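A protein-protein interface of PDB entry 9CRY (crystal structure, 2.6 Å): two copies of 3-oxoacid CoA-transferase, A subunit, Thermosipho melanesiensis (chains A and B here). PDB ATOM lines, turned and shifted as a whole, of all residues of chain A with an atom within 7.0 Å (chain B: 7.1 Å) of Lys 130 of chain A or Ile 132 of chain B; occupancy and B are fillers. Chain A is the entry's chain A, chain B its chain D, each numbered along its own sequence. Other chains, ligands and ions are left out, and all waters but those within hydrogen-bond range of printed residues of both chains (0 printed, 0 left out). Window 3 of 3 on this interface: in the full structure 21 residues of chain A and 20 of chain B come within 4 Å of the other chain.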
ATOM      1  N   LEU A 116     -13.926  -0.135  -9.885  1.00  0.00           N
ATOM      2  CA  LEU A 116     -13.365  -1.337 -10.484  1.00  0.00           C
ATOM      3  C   LEU A 116     -12.273  -1.885  -9.585  1.00  0.00           C
ATOM      4  O   LEU A 116     -11.319  -1.169  -9.261  1.00  0.00           O
ATOM      5  CB  LEU A 116     -12.780  -1.087 -11.878  1.00  0.00           C
ATOM      6  CG  LEU A 116     -13.463  -0.241 -12.941  1.00  0.00           C
ATOM      7  CD1 LEU A 116     -12.505  -0.084 -14.122  1.00  0.00           C
ATOM      8  CD2 LEU A 116     -14.748  -0.910 -13.385  1.00  0.00           C
ATOM      9  N   GLU A 126     -16.525 -13.299  -9.156  1.00  0.00           N
ATOM     10  CA  GLU A 126     -16.748 -12.755 -10.487  1.00  0.00           C
ATOM     11  C   GLU A 126     -18.145 -13.049 -11.023  1.00  0.00           C
ATOM     12  O   GLU A 126     -18.556 -12.451 -12.025  1.00  0.00           O
ATOM     13  CB  GLU A 126     -15.703 -13.323 -11.452  1.00  0.00           C
ATOM     14  CG  GLU A 126     -15.790 -12.732 -12.835  1.00  0.00           C
ATOM     15  CD  GLU A 126     -14.595 -13.090 -13.697  1.00  0.00           C
ATOM     16  OE1 GLU A 126     -13.481 -13.300 -13.154  1.00  0.00           O
ATOM     17  OE2 GLU A 126     -14.773 -13.154 -14.929  1.00  0.00           O
ATOM     18  N   LYS A 127     -18.900 -13.930 -10.383  1.00  0.00           N
ATOM     19  CA  LYS A 127     -20.194 -14.269 -10.950  1.00  0.00           C
ATOM     20  C   LYS A 127     -21.075 -13.035 -11.048  1.00  0.00           C
ATOM     21  O   LYS A 127     -21.146 -12.224 -10.118  1.00  0.00           O
ATOM     22  CB  LYS A 127     -20.924 -15.306 -10.109  1.00  0.00           C
ATOM     23  CG  LYS A 127     -21.189 -16.626 -10.802  1.00  0.00           C
ATOM     24  CD  LYS A 127     -20.853 -17.768  -9.857  1.00  0.00           C
ATOM     25  CE  LYS A 127     -21.831 -17.744  -8.677  1.00  0.00           C
ATOM     26  NZ  LYS A 127     -21.539 -18.796  -7.654  1.00  0.00           N
ATOM     27  N   ASP A 128     -21.753 -12.904 -12.184  1.00  0.00           N
ATOM     28  CA  ASP A 128     -22.765 -11.866 -12.368  1.00  0.00           C
ATOM     29  C   ASP A 128     -22.209 -10.484 -12.049  1.00  0.00           C
ATOM     30  O   ASP A 128     -22.902  -9.623 -11.497  1.00  0.00           O
ATOM     31  CB  ASP A 128     -23.993 -12.167 -11.499  1.00  0.00           C
ATOM     32  CG  ASP A 128     -24.649 -13.514 -11.854  1.00  0.00           C
ATOM     33  OD1 ASP A 128     -24.521 -13.973 -13.015  1.00  0.00           O
ATOM     34  OD2 ASP A 128     -25.247 -14.144 -10.954  1.00  0.00           O
ATOM     35  N   LYS A 129     -20.942 -10.265 -12.394  1.00  0.00           N
ATOM     36  CA  LYS A 129     -20.339  -8.947 -12.302  1.00  0.00           C
ATOM     37  C   LYS A 129     -19.832  -8.581 -13.685  1.00  0.00           C
ATOM     38  O   LYS A 129     -19.259  -9.419 -14.385  1.00  0.00           O
ATOM     39  CB  LYS A 129     -19.191  -8.893 -11.284  1.00  0.00           C
ATOM     40  CG  LYS A 129     -19.498  -9.467  -9.902  1.00  0.00           C
ATOM     41  CD  LYS A 129     -19.709  -8.370  -8.879  1.00  0.00           C
ATOM     42  CE  LYS A 129     -19.085  -8.765  -7.546  1.00  0.00           C
ATOM     43  NZ  LYS A 129     -19.940  -9.604  -6.676  1.00  0.00           N
ATOM     44  N   LYS A 130     -20.063  -7.341 -14.098  1.00  0.00           N
ATOM     45  CA  LYS A 130     -19.427  -6.881 -15.317  1.00  0.00           C
ATOM     46  C   LYS A 130     -17.918  -6.948 -15.108  1.00  0.00           C
ATOM     47  O   LYS A 130     -17.414  -6.683 -14.012  1.00  0.00           O
ATOM     48  CB  LYS A 130     -19.875  -5.459 -15.679  1.00  0.00           C
ATOM     49  CG  LYS A 130     -19.754  -5.174 -17.186  1.00  0.00           C
ATOM     50  CD  LYS A 130     -19.735  -3.679 -17.531  1.00  0.00           C
ATOM     51  CE  LYS A 130     -21.055  -3.240 -18.203  1.00  0.00           C
ATOM     52  NZ  LYS A 130     -20.939  -1.967 -19.000  1.00  0.00           N
ATOM     53  N   VAL A 131     -17.197  -7.362 -16.146  1.00  0.00           N
ATOM     54  CA  VAL A 131     -15.740  -7.373 -16.129  1.00  0.00           C
ATOM     55  C   VAL A 131     -15.258  -6.291 -17.073  1.00  0.00           C
ATOM     56  O   VAL A 131     -15.756  -6.167 -18.198  1.00  0.00           O
ATOM     57  CB  VAL A 131     -15.163  -8.736 -16.544  1.00  0.00           C
ATOM     58  CG1 VAL A 131     -13.671  -8.603 -16.843  1.00  0.00           C
ATOM     59  CG2 VAL A 131     -15.436  -9.768 -15.458  1.00  0.00           C
ATOM     60  N   ILE A 132     -14.281  -5.517 -16.621  1.00  0.00           N
ATOM     61  CA  ILE A 132     -13.724  -4.434 -17.417  1.00  0.00           C
ATOM     62  C   ILE A 132     -12.215  -4.557 -17.379  1.00  0.00           C
ATOM     63  O   ILE A 132     -11.624  -4.793 -16.314  1.00  0.00           O
ATOM     64  CB  ILE A 132     -14.179  -3.051 -16.916  1.00  0.00           C
ATOM     65  CG1 ILE A 132     -15.705  -3.030 -16.773  1.00  0.00           C
ATOM     66  CG2 ILE A 132     -13.705  -1.927 -17.854  1.00  0.00           C
ATOM     67  CD1 ILE A 132     -16.320  -1.644 -16.651  1.00  0.00           C
ATOM     68  N   TYR A 139     -10.772  -6.126 -14.188  1.00  0.00           N
ATOM     69  CA  TYR A 139     -11.313  -5.773 -12.881  1.00  0.00           C
ATOM     70  C   TYR A 139     -12.789  -6.114 -12.843  1.00  0.00           C
ATOM     71  O   TYR A 139     -13.482  -6.014 -13.857  1.00  0.00           O
ATOM     72  CB  TYR A 139     -11.162  -4.277 -12.560  1.00  0.00           C
ATOM     73  CG  TYR A 139      -9.778  -3.765 -12.756  1.00  0.00           C
ATOM     74  CD1 TYR A 139      -9.311  -3.478 -14.022  1.00  0.00           C
ATOM     75  CD2 TYR A 139      -8.911  -3.624 -11.675  1.00  0.00           C
ATOM     76  CE1 TYR A 139      -8.018  -3.031 -14.213  1.00  0.00           C
ATOM     77  CE2 TYR A 139      -7.623  -3.181 -11.852  1.00  0.00           C
ATOM     78  CZ  TYR A 139      -7.178  -2.885 -13.129  1.00  0.00           C
ATOM     79  OH  TYR A 139      -5.891  -2.437 -13.331  1.00  0.00           O
ATOM     80  N   LEU A 140     -13.281  -6.460 -11.659  1.00  0.00           N
ATOM     81  CA  LEU A 140     -14.718  -6.550 -11.478  1.00  0.00           C
ATOM     82  C   LEU A 140     -15.292  -5.151 -11.276  1.00  0.00           C
ATOM     83  O   LEU A 140     -14.770  -4.362 -10.482  1.00  0.00           O
ATOM     84  CB  LEU A 140     -15.071  -7.434 -10.281  1.00  0.00           C
ATOM     85  CG  LEU A 140     -14.334  -8.749 -10.092  1.00  0.00           C
ATOM     86  CD1 LEU A 140     -14.945  -9.574  -8.982  1.00  0.00           C
ATOM     87  CD2 LEU A 140     -14.370  -9.484 -11.416  1.00  0.00           C
ATOM     88  N   LEU A 141     -16.359  -4.838 -12.002  1.00  0.00           N
ATOM     89  CA  LEU A 141     -17.169  -3.676 -11.669  1.00  0.00           C
ATOM     90  C   LEU A 141     -17.952  -4.012 -10.410  1.00  0.00           C
ATOM     91  O   LEU A 141     -18.648  -5.030 -10.364  1.00  0.00           O
ATOM     92  CB  LEU A 141     -18.108  -3.324 -12.815  1.00  0.00           C
ATOM     93  CG  LEU A 141     -19.043  -2.158 -12.511  1.00  0.00           C
ATOM     94  CD1 LEU A 141     -18.254  -0.974 -11.996  1.00  0.00           C
ATOM     95  CD2 LEU A 141     -19.859  -1.777 -13.733  1.00  0.00           C
ATOM     96  N   GLU A 142     -17.789  -3.199  -9.368  1.00  0.00           N
ATOM     97  CA  GLU A 142     -18.470  -3.392  -8.100  1.00  0.00           C
ATOM     98  C   GLU A 142     -19.333  -2.167  -7.840  1.00  0.00           C
ATOM     99  O   GLU A 142     -18.935  -1.039  -8.143  1.00  0.00           O
ATOM    100  CB  GLU A 142     -17.462  -3.620  -6.988  1.00  0.00           C
ATOM    101  CG  GLU A 142     -16.719  -4.910  -7.186  1.00  0.00           C
ATOM    102  CD  GLU A 142     -17.499  -6.076  -6.665  1.00  0.00           C
ATOM    103  OE1 GLU A 142     -18.711  -5.902  -6.429  1.00  0.00           O
ATOM    104  OE2 GLU A 142     -16.914  -7.170  -6.496  1.00  0.00           O
ATOM    105  N   LEU A 143     -20.513  -2.390  -7.289  1.00  0.00           N
ATOM    106  CA  LEU A 143     -21.509  -1.344  -7.393  1.00  0.00           C
ATOM    107  C   LEU A 143     -21.898  -0.798  -6.034  1.00  0.00           C
ATOM    108  O   LEU A 143     -21.763  -1.479  -5.014  1.00  0.00           O
ATOM    109  CB  LEU A 143     -22.757  -1.853  -8.118  1.00  0.00           C
ATOM    110  CG  LEU A 143     -22.545  -2.262  -9.576  1.00  0.00           C
ATOM    111  CD1 LEU A 143     -23.674  -3.209  -9.952  1.00  0.00           C
ATOM    112  CD2 LEU A 143     -22.514  -1.064 -10.507  1.00  0.00           C
ATOM    113  N   LEU B 116     -16.470   5.187 -11.394  1.00  0.00           N
ATOM    114  CA  LEU B 116     -17.499   5.736 -12.248  1.00  0.00           C
ATOM    115  C   LEU B 116     -18.099   6.960 -11.576  1.00  0.00           C
ATOM    116  O   LEU B 116     -18.455   6.899 -10.403  1.00  0.00           O
ATOM    117  CB  LEU B 116     -18.583   4.707 -12.518  1.00  0.00           C
ATOM    118  CG  LEU B 116     -18.188   3.474 -13.342  1.00  0.00           C
ATOM    119  CD1 LEU B 116     -17.059   2.590 -12.773  1.00  0.00           C
ATOM    120  CD2 LEU B 116     -19.425   2.699 -13.644  1.00  0.00           C
ATOM    121  N   VAL B 121     -20.677  14.102 -17.155  1.00  0.00           N
ATOM    122  CA  VAL B 121     -21.592  13.504 -18.118  1.00  0.00           C
ATOM    123  C   VAL B 121     -22.271  14.601 -18.920  1.00  0.00           C
ATOM    124  O   VAL B 121     -22.869  15.524 -18.356  1.00  0.00           O
ATOM    125  CB  VAL B 121     -22.627  12.620 -17.401  1.00  0.00           C
ATOM    126  CG1 VAL B 121     -23.692  12.157 -18.395  1.00  0.00           C
ATOM    127  CG2 VAL B 121     -21.954  11.437 -16.712  1.00  0.00           C
ATOM    128  N   LYS B 129     -14.138   9.276 -23.227  1.00  0.00           N
ATOM    129  CA  LYS B 129     -14.354   8.467 -22.034  1.00  0.00           C
ATOM    130  C   LYS B 129     -15.355   7.363 -22.344  1.00  0.00           C
ATOM    131  O   LYS B 129     -16.331   7.590 -23.068  1.00  0.00           O
ATOM    132  CB  LYS B 129     -14.886   9.298 -20.838  1.00  0.00           C
ATOM    133  CG  LYS B 129     -14.165  10.598 -20.498  1.00  0.00           C
ATOM    134  CD  LYS B 129     -12.854  10.365 -19.769  1.00  0.00           C
ATOM    135  CE  LYS B 129     -12.628  11.465 -18.709  1.00  0.00           C
ATOM    136  NZ  LYS B 129     -12.167  12.793 -19.225  1.00  0.00           N
ATOM    137  N   LYS B 130     -15.114   6.169 -21.801  1.00  0.00           N
ATOM    138  CA  LYS B 130     -16.154   5.149 -21.785  1.00  0.00           C
ATOM    139  C   LYS B 130     -17.304   5.619 -20.905  1.00  0.00           C
ATOM    140  O   LYS B 130     -17.086   6.186 -19.831  1.00  0.00           O
ATOM    141  CB  LYS B 130     -15.618   3.821 -21.254  1.00  0.00           C
ATOM    142  CG  LYS B 130     -16.689   2.736 -21.142  1.00  0.00           C
ATOM    143  CD  LYS B 130     -16.142   1.437 -20.531  1.00  0.00           C
ATOM    144  CE  LYS B 130     -16.706   0.173 -21.206  1.00  0.00           C
ATOM    145  NZ  LYS B 130     -15.687  -0.936 -21.313  1.00  0.00           N
ATOM    146  N   VAL B 131     -18.532   5.365 -21.354  1.00  0.00           N
ATOM    147  CA  VAL B 131     -19.740   5.683 -20.597  1.00  0.00           C
ATOM    148  C   VAL B 131     -20.346   4.374 -20.120  1.00  0.00           C
ATOM    149  O   VAL B 131     -20.334   3.380 -20.853  1.00  0.00           O
ATOM    150  CB  VAL B 131     -20.758   6.479 -21.432  1.00  0.00           C
ATOM    151  CG1 VAL B 131     -22.046   6.634 -20.651  1.00  0.00           C
ATOM    152  CG2 VAL B 131     -20.200   7.853 -21.801  1.00  0.00           C
ATOM    153  N   ILE B 132     -20.833   4.353 -18.879  1.00  0.00           N
ATOM    154  CA  ILE B 132     -21.377   3.135 -18.289  1.00  0.00           C
ATOM    155  C   ILE B 132     -22.678   3.457 -17.569  1.00  0.00           C
ATOM    156  O   ILE B 132     -22.732   4.400 -16.775  1.00  0.00           O
ATOM    157  CB  ILE B 132     -20.390   2.485 -17.303  1.00  0.00           C
ATOM    158  CG1 ILE B 132     -19.011   2.312 -17.942  1.00  0.00           C
ATOM    159  CG2 ILE B 132     -20.971   1.134 -16.816  1.00  0.00           C
ATOM    160  CD1 ILE B 132     -18.163   1.279 -17.247  1.00  0.00           C
ATOM    161  N   GLU B 133     -23.714   2.660 -17.823  1.00  0.00           N
ATOM    162  CA  GLU B 133     -25.023   2.842 -17.200  1.00  0.00           C
ATOM    163  C   GLU B 133     -25.196   1.840 -16.065  1.00  0.00           C
ATOM    164  O   GLU B 133     -24.932   0.639 -16.233  1.00  0.00           O
ATOM    165  CB  GLU B 133     -26.145   2.676 -18.223  1.00  0.00           C
ATOM    166  CG  GLU B 133     -26.511   3.956 -18.966  1.00  0.00           C
ATOM    167  CD  GLU B 133     -28.016   4.175 -19.059  1.00  0.00           C
ATOM    168  OE1 GLU B 133     -28.460   5.200 -19.582  1.00  0.00           O
ATOM    169  OE2 GLU B 133     -28.792   3.325 -18.611  1.00  0.00           O
ATOM    170  N   VAL B 134     -25.616   2.345 -14.912  1.00  0.00           N
ATOM    171  CA  VAL B 134     -25.891   1.550 -13.717  1.00  0.00           C
ATOM    172  C   VAL B 134     -27.231   2.028 -13.189  1.00  0.00           C
ATOM    173  O   VAL B 134     -27.363   3.203 -12.817  1.00  0.00           O
ATOM    174  CB  VAL B 134     -24.796   1.724 -12.652  1.00  0.00           C
ATOM    175  CG1 VAL B 134     -25.218   1.057 -11.359  1.00  0.00           C
ATOM    176  CG2 VAL B 134     -23.438   1.171 -13.147  1.00  0.00           C
ATOM    177  N   LYS B 137     -28.769   5.339 -14.692  1.00  0.00           N
ATOM    178  CA  LYS B 137     -27.970   6.555 -14.635  1.00  0.00           C
ATOM    179  C   LYS B 137     -26.667   6.326 -15.404  1.00  0.00           C
ATOM    180  O   LYS B 137     -26.069   5.245 -15.336  1.00  0.00           O
ATOM    181  CB  LYS B 137     -27.682   6.996 -13.199  1.00  0.00           C
ATOM    182  CG  LYS B 137     -27.204   8.458 -13.173  1.00  0.00           C
ATOM    183  CD  LYS B 137     -27.258   9.213 -11.845  1.00  0.00           C
ATOM    184  CE  LYS B 137     -26.712  10.627 -12.124  1.00  0.00           C
ATOM    185  NZ  LYS B 137     -26.544  11.553 -10.960  1.00  0.00           N
ATOM    186  N   LYS B 138     -26.250   7.332 -16.170  1.00  0.00           N
ATOM    187  CA  LYS B 138     -24.993   7.292 -16.920  1.00  0.00           C
ATOM    188  C   LYS B 138     -23.841   7.768 -16.036  1.00  0.00           C
ATOM    189  O   LYS B 138     -23.995   8.705 -15.236  1.00  0.00           O
ATOM    190  CB  LYS B 138     -25.091   8.186 -18.153  1.00  0.00           C
ATOM    191  CG  LYS B 138     -25.888   7.693 -19.342  1.00  0.00           C
ATOM    192  CD  LYS B 138     -25.957   8.877 -20.325  1.00  0.00           C
ATOM    193  CE  LYS B 138     -27.261   9.733 -20.009  1.00  0.00           C
ATOM    194  NZ  LYS B 138     -27.563  10.753 -21.074  1.00  0.00           N
ATOM    195  N   TYR B 139     -22.687   7.128 -16.191  1.00  0.00           N
ATOM    196  CA  TYR B 139     -21.486   7.556 -15.504  1.00  0.00           C
ATOM    197  C   TYR B 139     -20.328   7.548 -16.483  1.00  0.00           C
ATOM    198  O   TYR B 139     -20.321   6.792 -17.456  1.00  0.00           O
ATOM    199  CB  TYR B 139     -21.162   6.653 -14.312  1.00  0.00           C
ATOM    200  CG  TYR B 139     -22.253   6.615 -13.282  1.00  0.00           C
ATOM    201  CD1 TYR B 139     -23.259   5.672 -13.373  1.00  0.00           C
ATOM    202  CD2 TYR B 139     -22.290   7.528 -12.231  1.00  0.00           C
ATOM    203  CE1 TYR B 139     -24.264   5.619 -12.447  1.00  0.00           C
ATOM    204  CE2 TYR B 139     -23.295   7.480 -11.299  1.00  0.00           C
ATOM    205  CZ  TYR B 139     -24.281   6.521 -11.416  1.00  0.00           C
ATOM    206  OH  TYR B 139     -25.290   6.460 -10.487  1.00  0.00           O
ATOM    207  N   LEU B 140     -19.346   8.389 -16.213  1.00  0.00           N
ATOM    208  CA  LEU B 140     -18.063   8.268 -16.878  1.00  0.00           C
ATOM    209  C   LEU B 140     -17.176   7.269 -16.142  1.00  0.00           C
ATOM    210  O   LEU B 140     -17.048   7.311 -14.913  1.00  0.00           O
ATOM    211  CB  LEU B 140     -17.381   9.627 -16.958  1.00  0.00           C
ATOM    212  CG  LEU B 140     -18.196  10.764 -17.571  1.00  0.00           C
ATOM    213  CD1 LEU B 140     -17.332  12.004 -17.842  1.00  0.00           C
ATOM    214  CD2 LEU B 140     -18.890  10.303 -18.835  1.00  0.00           C
ATOM    215  N   LEU B 141     -16.534   6.393 -16.908  1.00  0.00           N
ATOM    216  CA  LEU B 141     -15.428   5.602 -16.384  1.00  0.00           C
ATOM    217  C   LEU B 141     -14.190   6.483 -16.356  1.00  0.00           C
ATOM    218  O   LEU B 141     -13.758   6.977 -17.401  1.00  0.00           O
ATOM    219  CB  LEU B 141     -15.180   4.353 -17.224  1.00  0.00           C
ATOM    220  CG  LEU B 141     -13.990   3.518 -16.730  1.00  0.00           C
ATOM    221  CD1 LEU B 141     -14.143   3.146 -15.245  1.00  0.00           C
ATOM    222  CD2 LEU B 141     -13.772   2.277 -17.605  1.00  0.00           C
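Of the 13 printed residues of chain A, 5 touch a printed residue of chain B. Printed residues of chain A that touch a printed residue of chain B: Leu 116, Lys 130, Ile 132, Leu 141 and Leu 143. Hydrophobic or aromatic side chains of chain A within 4 Å of the printed part of chain B: Leu 116, Ile 132, Leu 141 and Leu 143. Of the 13 printed residues of chain B, 4 touch a printed residue of chain A. Hydrophobic or aromatic side chains of chain B within 4 Å of the printed part of chain A: Leu 116, Ile 132, Val 134 and Leu 141.
The backbone carbonyl oxygen (O) of Lys 130 of chain A lies within hydrogen-bond range of the backbone NH (N) of Leu 141 of chain A (2.9 Å). The backbone carbonyl oxygen of Lys 130 of chain B is in hydrogen-bond range of the backbone NH of Leu 141 of chain B (3.0 Å). The backbone NH of Tyr 139 of chain A sits at hydrogen-bond distance from the backbone carbonyl oxygen of Ile 132 of chain A, at 2.7 Å. N of Tyr 139 of chain B sits at hydrogen-bond distance from O of Ile 132 of chain B (2.8 Å).
Leu 116 of chain A touches Leu 141 of chain B, and with the chains exchanged Leu 141 of chain A touches Leu 116 of chain B. Lys 130 of chain A touches Ile 132 of chain B, but with the chains exchanged Ile 132 of chain A does not touch Lys 130 of chain B (4.1 Å). Ile 132 of chain A touches its own counterpart, Ile 132 of chain B. Of the 5 pairs that touch across the chains among the printed residues, 3 have their exchanged pair printed and touching as well.
Leu 116 of chain A touches Leu 141 of chain B. CG2 of Ile 132 of chain B touches NZ of Lys 130 of chain A (3.8 Å). Ile 132 of chain B touches Ile 132 of chain A (CD1 to CD1, 3.5 Å). Leu 141 of chain A touches Leu 116 of chain B. CD2 of Leu 143 of chain A touches CG1 of Val 134 of chain B, 3.5 Å away.
Printed residues of chain B within 4 Å of Leu 116 of chain A: Leu 141 (3.8 Å). Lys 127 of chain A touches none of the printed residues of chain B. Of chain B, only Ile 132 comes within 4 Å of Lys 130 of chain A. Of the printed residues of chain B, Ile 132 of chain A touches Ile 132. Of the printed residues of chain B, Leu 143 of chain A touches Val 134. Printed residues of chain A within 4 Å of Ile 132 of chain B: Lys 130 (3.8 Å) and Ile 132 (3.5 Å). Printed residues of chain A within 4 Å of Val 134 of chain B: Leu 143. The nearest residue of chain B that does not touch Lys 130 of chain A is Lys 130 of chain B (5.2 Å). The nearest residue of chain A that does not touch Ile 132 of chain B is Leu 141 of chain A (4.4 Å). The nearest printed residue of chain A that does not touch Leu 116 of chain B is Leu 116 of chain A (4.2 Å).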
